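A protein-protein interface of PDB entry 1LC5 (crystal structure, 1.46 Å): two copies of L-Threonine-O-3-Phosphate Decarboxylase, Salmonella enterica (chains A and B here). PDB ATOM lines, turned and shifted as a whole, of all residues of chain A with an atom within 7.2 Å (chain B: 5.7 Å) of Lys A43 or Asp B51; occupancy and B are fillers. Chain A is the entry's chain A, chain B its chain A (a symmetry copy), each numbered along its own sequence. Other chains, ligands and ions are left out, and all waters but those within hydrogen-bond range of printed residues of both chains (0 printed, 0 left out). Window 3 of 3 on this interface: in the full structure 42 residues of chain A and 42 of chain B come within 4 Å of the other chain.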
ATOM      1  N   GLY A  37     -14.983 -33.527  24.359  1.00  0.00           N
ATOM      2  CA  GLY A  37     -15.976 -32.726  23.668  1.00  0.00           C
ATOM      3  C   GLY A  37     -15.434 -32.155  22.378  1.00  0.00           C
ATOM      4  O   GLY A  37     -15.004 -32.905  21.512  1.00  0.00           O
ATOM      5  N   MET A  38     -15.466 -30.833  22.254  1.00  0.00           N
ATOM      6  CA  MET A  38     -14.966 -30.149  21.060  1.00  0.00           C
ATOM      7  C   MET A  38     -14.252 -28.866  21.501  1.00  0.00           C
ATOM      8  O   MET A  38     -14.722 -28.189  22.410  1.00  0.00           O
ATOM      9  CB  MET A  38     -16.142 -29.772  20.158  1.00  0.00           C
ATOM     10  CG  MET A  38     -15.728 -29.157  18.839  1.00  0.00           C
ATOM     11  SD  MET A  38     -17.104 -28.385  17.940  1.00  0.00           S
ATOM     12  CE  MET A  38     -18.218 -29.809  17.683  1.00  0.00           C
ATOM     13  N   PRO A  39     -13.110 -28.521  20.882  1.00  0.00           N
ATOM     14  CA  PRO A  39     -12.382 -27.300  21.251  1.00  0.00           C
ATOM     15  C   PRO A  39     -13.272 -26.072  21.073  1.00  0.00           C
ATOM     16  O   PRO A  39     -14.055 -25.988  20.117  1.00  0.00           O
ATOM     17  CB  PRO A  39     -11.203 -27.293  20.278  1.00  0.00           C
ATOM     18  CG  PRO A  39     -10.986 -28.749  19.991  1.00  0.00           C
ATOM     19  CD  PRO A  39     -12.371 -29.292  19.866  1.00  0.00           C
ATOM     20  N   VAL A  40     -13.175 -25.126  22.005  1.00  0.00           N
ATOM     21  CA  VAL A  40     -13.964 -23.902  21.926  1.00  0.00           C
ATOM     22  C   VAL A  40     -13.574 -23.093  20.688  1.00  0.00           C
ATOM     23  O   VAL A  40     -14.423 -22.471  20.052  1.00  0.00           O
ATOM     24  CB  VAL A  40     -13.765 -23.031  23.190  1.00  0.00           C
ATOM     25  CG1 VAL A  40     -14.562 -21.734  23.069  1.00  0.00           C
ATOM     26  CG2 VAL A  40     -14.209 -23.806  24.416  1.00  0.00           C
ATOM     27  N   SER A  41     -12.291 -23.116  20.334  1.00  0.00           N
ATOM     28  CA  SER A  41     -11.820 -22.381  19.162  1.00  0.00           C
ATOM     29  C   SER A  41     -12.504 -22.902  17.898  1.00  0.00           C
ATOM     30  O   SER A  41     -12.815 -22.146  16.978  1.00  0.00           O
ATOM     31  CB  SER A  41     -10.303 -22.524  19.016  1.00  0.00           C
ATOM     32  OG  SER A  41      -9.927 -23.877  18.821  1.00  0.00           O
ATOM     33  N   VAL A  42     -12.760 -24.200  17.865  1.00  0.00           N
ATOM     34  CA  VAL A  42     -13.387 -24.797  16.699  1.00  0.00           C
ATOM     35  C   VAL A  42     -14.896 -24.562  16.619  1.00  0.00           C
ATOM     36  O   VAL A  42     -15.441 -24.176  15.571  1.00  0.00           O
ATOM     37  CB  VAL A  42     -13.112 -26.314  16.658  1.00  0.00           C
ATOM     38  CG1 VAL A  42     -13.888 -26.946  15.522  1.00  0.00           C
ATOM     39  CG2 VAL A  42     -11.625 -26.563  16.491  1.00  0.00           C
ATOM     40  N   LYS A  43     -15.598 -24.783  17.715  1.00  0.00           N
ATOM     41  CA  LYS A  43     -17.037 -24.618  17.687  1.00  0.00           C
ATOM     42  C   LYS A  43     -17.444 -23.202  17.269  1.00  0.00           C
ATOM     43  O   LYS A  43     -18.293 -23.017  16.399  1.00  0.00           O
ATOM     44  CB  LYS A  43     -17.619 -24.930  19.068  1.00  0.00           C
ATOM     45  CG  LYS A  43     -19.137 -24.942  19.078  1.00  0.00           C
ATOM     46  CD  LYS A  43     -19.701 -25.302  20.452  1.00  0.00           C
ATOM     47  CE  LYS A  43     -19.691 -26.811  20.696  1.00  0.00           C
ATOM     48  NZ  LYS A  43     -20.252 -27.172  22.033  1.00  0.00           N
ATOM     49  N   ARG A  44     -16.818 -22.216  17.896  1.00  0.00           N
ATOM     50  CA  ARG A  44     -17.114 -20.820  17.600  1.00  0.00           C
ATOM     51  C   ARG A  44     -16.836 -20.483  16.138  1.00  0.00           C
ATOM     52  O   ARG A  44     -17.688 -19.908  15.459  1.00  0.00           O
ATOM     53  CB  ARG A  44     -16.288 -19.912  18.515  1.00  0.00           C
ATOM     54  N   ALA A  45     -15.645 -20.838  15.665  1.00  0.00           N
ATOM     55  CA  ALA A  45     -15.253 -20.557  14.289  1.00  0.00           C
ATOM     56  C   ALA A  45     -16.250 -21.133  13.278  1.00  0.00           C
ATOM     57  O   ALA A  45     -16.710 -20.432  12.372  1.00  0.00           O
ATOM     58  CB  ALA A  45     -13.856 -21.088  14.023  1.00  0.00           C
ATOM     59  N   LEU A  46     -16.599 -22.405  13.433  1.00  0.00           N
ATOM     60  CA  LEU A  46     -17.540 -23.032  12.510  1.00  0.00           C
ATOM     61  C   LEU A  46     -18.909 -22.354  12.529  1.00  0.00           C
ATOM     62  O   LEU A  46     -19.500 -22.077  11.485  1.00  0.00           O
ATOM     63  CB  LEU A  46     -17.675 -24.526  12.842  1.00  0.00           C
ATOM     64  CG  LEU A  46     -16.769 -25.504  12.060  1.00  0.00           C
ATOM     65  CD1 LEU A  46     -15.338 -25.018  11.944  1.00  0.00           C
ATOM     66  CD2 LEU A  46     -16.828 -26.845  12.772  1.00  0.00           C
ATOM     67  N   ILE A  47     -19.424 -22.080  13.720  1.00  0.00           N
ATOM     68  CA  ILE A  47     -20.717 -21.437  13.828  1.00  0.00           C
ATOM     69  C   ILE A  47     -20.736 -20.025  13.233  1.00  0.00           C
ATOM     70  O   ILE A  47     -21.635 -19.675  12.475  1.00  0.00           O
ATOM     71  CB  ILE A  47     -21.149 -21.346  15.294  1.00  0.00           C
ATOM     72  CG1 ILE A  47     -21.442 -22.743  15.831  1.00  0.00           C
ATOM     73  CG2 ILE A  47     -22.384 -20.462  15.417  1.00  0.00           C
ATOM     74  CD1 ILE A  47     -22.575 -23.428  15.110  1.00  0.00           C
ATOM     75  N   ASP A  48     -19.724 -19.235  13.550  1.00  0.00           N
ATOM     76  CA  ASP A  48     -19.690 -17.858  13.061  1.00  0.00           C
ATOM     77  C   ASP A  48     -19.288 -17.695  11.598  1.00  0.00           C
ATOM     78  O   ASP A  48     -19.377 -16.598  11.055  1.00  0.00           O
ATOM     79  CB  ASP A  48     -18.752 -17.026  13.923  1.00  0.00           C
ATOM     80  CG  ASP A  48     -19.220 -16.916  15.373  1.00  0.00           C
ATOM     81  OD1 ASP A  48     -20.437 -17.044  15.636  1.00  0.00           O
ATOM     82  OD2 ASP A  48     -18.353 -16.685  16.238  1.00  0.00           O
ATOM     83  N   ASN A  49     -18.871 -18.775  10.946  1.00  0.00           N
ATOM     84  CA  ASN A  49     -18.430 -18.658   9.557  1.00  0.00           C
ATOM     85  C   ASN A  49     -19.037 -19.735   8.659  1.00  0.00           C
ATOM     86  O   ASN A  49     -18.488 -20.063   7.604  1.00  0.00           O
ATOM     87  CB  ASN A  49     -16.905 -18.769   9.488  1.00  0.00           C
ATOM     88  CG  ASN A  49     -16.195 -17.662  10.239  1.00  0.00           C
ATOM     89  OD1 ASN A  49     -16.036 -16.554   9.728  1.00  0.00           O
ATOM     90  ND2 ASN A  49     -15.762 -17.957  11.458  1.00  0.00           N
ATOM     91  N   ALA A 219     -10.619 -33.781  18.417  1.00  0.00           N
ATOM     92  CA  ALA A 219     -11.960 -34.346  18.315  1.00  0.00           C
ATOM     93  C   ALA A 219     -12.765 -33.851  17.117  1.00  0.00           C
ATOM     94  O   ALA A 219     -13.950 -33.476  17.227  1.00  0.00           O
ATOM     95  CB  ALA A 219     -12.738 -34.105  19.636  1.00  0.00           C
ATOM     96  N   ALA A 255     -11.132 -25.003  11.058  1.00  0.00           N
ATOM     97  CA  ALA A 255     -10.729 -25.608  12.336  1.00  0.00           C
ATOM     98  C   ALA A 255      -9.207 -25.744  12.451  1.00  0.00           C
ATOM     99  O   ALA A 255      -8.630 -25.478  13.515  1.00  0.00           O
ATOM    100  CB  ALA A 255     -11.400 -26.975  12.495  1.00  0.00           C
ATOM    101  N   VAL A 258      -7.303 -22.553  13.706  1.00  0.00           N
ATOM    102  CA  VAL A 258      -7.406 -22.070  15.072  1.00  0.00           C
ATOM    103  C   VAL A 258      -7.122 -23.093  16.152  1.00  0.00           C
ATOM    104  O   VAL A 258      -6.673 -22.747  17.242  1.00  0.00           O
ATOM    105  CB  VAL A 258      -8.806 -21.500  15.340  1.00  0.00           C
ATOM    106  CG1 VAL A 258      -9.033 -20.291  14.469  1.00  0.00           C
ATOM    107  CG2 VAL A 258      -9.880 -22.539  15.111  1.00  0.00           C
ATOM    108  N   ASP A 262      -5.283 -23.407  20.528  1.00  0.00           N
ATOM    109  CA  ASP A 262      -6.249 -23.563  21.619  1.00  0.00           C
ATOM    110  C   ASP A 262      -5.542 -24.143  22.845  1.00  0.00           C
ATOM    111  O   ASP A 262      -5.600 -25.348  23.111  1.00  0.00           O
ATOM    112  CB  ASP A 262      -7.401 -24.474  21.174  1.00  0.00           C
ATOM    113  CG  ASP A 262      -8.659 -24.298  22.021  1.00  0.00           C
ATOM    114  OD1 ASP A 262      -9.771 -24.363  21.459  1.00  0.00           O
ATOM    115  OD2 ASP A 262      -8.553 -24.105  23.251  1.00  0.00           O
ATOM    116  N   ASN B  49     -26.591 -30.037  14.504  1.00  0.00           N
ATOM    117  CA  ASN B  49     -25.905 -31.320  14.646  1.00  0.00           C
ATOM    118  C   ASN B  49     -24.387 -31.186  14.537  1.00  0.00           C
ATOM    119  O   ASN B  49     -23.688 -32.149  14.212  1.00  0.00           O
ATOM    120  CB  ASN B  49     -26.388 -32.287  13.564  1.00  0.00           C
ATOM    121  CG  ASN B  49     -27.867 -32.599  13.663  1.00  0.00           C
ATOM    122  OD1 ASN B  49     -28.282 -33.441  14.457  1.00  0.00           O
ATOM    123  ND2 ASN B  49     -28.670 -31.920  12.853  1.00  0.00           N
ATOM    124  N   LEU B  50     -23.869 -30.010  14.812  1.00  0.00           N
ATOM    125  CA  LEU B  50     -22.448 -29.766  14.707  1.00  0.00           C
ATOM    126  C   LEU B  50     -21.581 -30.755  15.474  1.00  0.00           C
ATOM    127  O   LEU B  50     -20.484 -31.097  15.022  1.00  0.00           O
ATOM    128  CB  LEU B  50     -22.131 -28.338  15.159  1.00  0.00           C
ATOM    129  CG  LEU B  50     -20.779 -27.775  14.747  1.00  0.00           C
ATOM    130  CD1 LEU B  50     -20.713 -27.652  13.221  1.00  0.00           C
ATOM    131  CD2 LEU B  50     -20.598 -26.414  15.395  1.00  0.00           C
ATOM    132  N   ASP B  51     -22.068 -31.230  16.621  1.00  0.00           N
ATOM    133  CA  ASP B  51     -21.277 -32.148  17.427  1.00  0.00           C
ATOM    134  C   ASP B  51     -21.000 -33.478  16.751  1.00  0.00           C
ATOM    135  O   ASP B  51     -20.164 -34.261  17.229  1.00  0.00           O
ATOM    136  CB  ASP B  51     -21.938 -32.388  18.794  1.00  0.00           C
ATOM    137  CG  ASP B  51     -22.055 -31.111  19.625  1.00  0.00           C
ATOM    138  OD1 ASP B  51     -21.201 -30.205  19.488  1.00  0.00           O
ATOM    139  OD2 ASP B  51     -23.003 -31.029  20.438  1.00  0.00           O
ATOM    140  N   CYS B  52     -21.679 -33.751  15.633  1.00  0.00           N
ATOM    141  CA  CYS B  52     -21.421 -35.009  14.957  1.00  0.00           C
ATOM    142  C   CYS B  52     -19.985 -35.051  14.415  1.00  0.00           C
ATOM    143  O   CYS B  52     -19.495 -36.134  14.088  1.00  0.00           O
ATOM    144  CB  CYS B  52     -22.427 -35.276  13.825  1.00  0.00           C
ATOM    145  SG  CYS B  52     -22.163 -34.336  12.325  1.00  0.00           S
ATOM    146  N   ILE B  53     -19.292 -33.916  14.359  1.00  0.00           N
ATOM    147  CA  ILE B  53     -17.918 -33.964  13.871  1.00  0.00           C
ATOM    148  C   ILE B  53     -16.968 -34.615  14.862  1.00  0.00           C
ATOM    149  O   ILE B  53     -15.816 -34.899  14.545  1.00  0.00           O
ATOM    150  CB  ILE B  53     -17.372 -32.574  13.476  1.00  0.00           C
ATOM    151  CG1 ILE B  53     -17.243 -31.665  14.692  1.00  0.00           C
ATOM    152  CG2 ILE B  53     -18.286 -31.967  12.390  1.00  0.00           C
ATOM    153  CD1 ILE B  53     -16.616 -30.278  14.368  1.00  0.00           C
ATOM    154  N   GLU B  54     -17.457 -34.868  16.079  1.00  0.00           N
ATOM    155  CA  GLU B  54     -16.627 -35.526  17.096  1.00  0.00           C
ATOM    156  C   GLU B  54     -16.444 -37.019  16.849  1.00  0.00           C
ATOM    157  O   GLU B  54     -15.666 -37.665  17.571  1.00  0.00           O
ATOM    158  CB  GLU B  54     -17.227 -35.317  18.498  1.00  0.00           C
ATOM    159  CG  GLU B  54     -17.242 -33.846  18.869  1.00  0.00           C
ATOM    160  CD  GLU B  54     -17.916 -33.526  20.184  1.00  0.00           C
ATOM    161  OE1 GLU B  54     -18.242 -34.440  20.954  1.00  0.00           O
ATOM    162  OE2 GLU B  54     -18.104 -32.322  20.428  1.00  0.00           O
ATOM    163  N   ARG B  55     -17.141 -37.564  15.852  1.00  0.00           N
ATOM    164  CA  ARG B  55     -17.021 -38.976  15.499  1.00  0.00           C
ATOM    165  C   ARG B  55     -16.727 -39.132  14.013  1.00  0.00           C
ATOM    166  O   ARG B  55     -17.079 -38.265  13.202  1.00  0.00           O
ATOM    167  CB  ARG B  55     -18.348 -39.707  15.787  1.00  0.00           C
ATOM    168  CG  ARG B  55     -18.729 -39.663  17.249  1.00  0.00           C
ATOM    169  CD  ARG B  55     -20.157 -40.133  17.513  1.00  0.00           C
ATOM    170  NE  ARG B  55     -21.191 -39.182  17.094  1.00  0.00           N
ATOM    171  CZ  ARG B  55     -21.912 -39.309  15.987  1.00  0.00           C
ATOM    172  NH1 ARG B  55     -21.706 -40.338  15.181  1.00  0.00           N
ATOM    173  NH2 ARG B  55     -22.871 -38.435  15.706  1.00  0.00           N
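Of the 17 printed residues of chain A, 6 touch a printed residue of chain B. Hydrophobic or aromatic side chains of chain A within 4 Å of the printed part of chain B: Met A38, Leu A46 and Ile A47. Among the printed residues, 11 pairs touch across the chains. Among the printed residues, no Asp or Glu carboxylate lies within 4 Å of a Lys or Arg side-chain nitrogen of the other chain.
O of Gly A37 lies close to OE2 of Glu B54.
Position printed for both chains: 49.
Of the printed residues of chain B, Gly A37 touches Glu B54 (3.3 Å). Printed residues of chain B within 4 Å of Met A38: Leu B50 (3.7 Å), Asp B51 (3.5 Å), Ile B53 (3.7 Å) and Glu B54 (3.2 Å). Of chain B, only Asp B51 (3.9 Å) comes within 4 Å of Lys A43. Of the printed residues of chain B, Ile A47 touches Leu B50 (3.6 Å). Val A258 touches none of the printed residues of chain B. Of chain A, only Met A38 and Lys A43 come within 4 Å of Asp B51. Of the printed residues of chain A, Ile B53 touches Met A38, Leu A46 and Ala A219. The nearest residue of chain B that does not touch Lys A43 is Leu B50 (4.2 Å). The nearest printed residue of chain A that does not touch Glu B54 is Lys A43 (5.7 Å).
Among the printed residues, merely in contact across the chains: Met A38 with Leu B50 (3.7 Å), Met A38 with Asp B51 (3.5 Å), Met A38 with Ile B53 (3.7 Å), Met A38 with Glu B54 (3.2 Å), Lys A43 with Asp B51 (3.9 Å), Leu A46 with Leu B50 (3.99 Å), Leu A46 with Ile B53 (3.8 Å), Ile A47 with Leu B50 (3.6 Å), Ala A219 with Ile B53 (3.6 Å) and Ala A219 with Glu B54 (3.4 Å).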
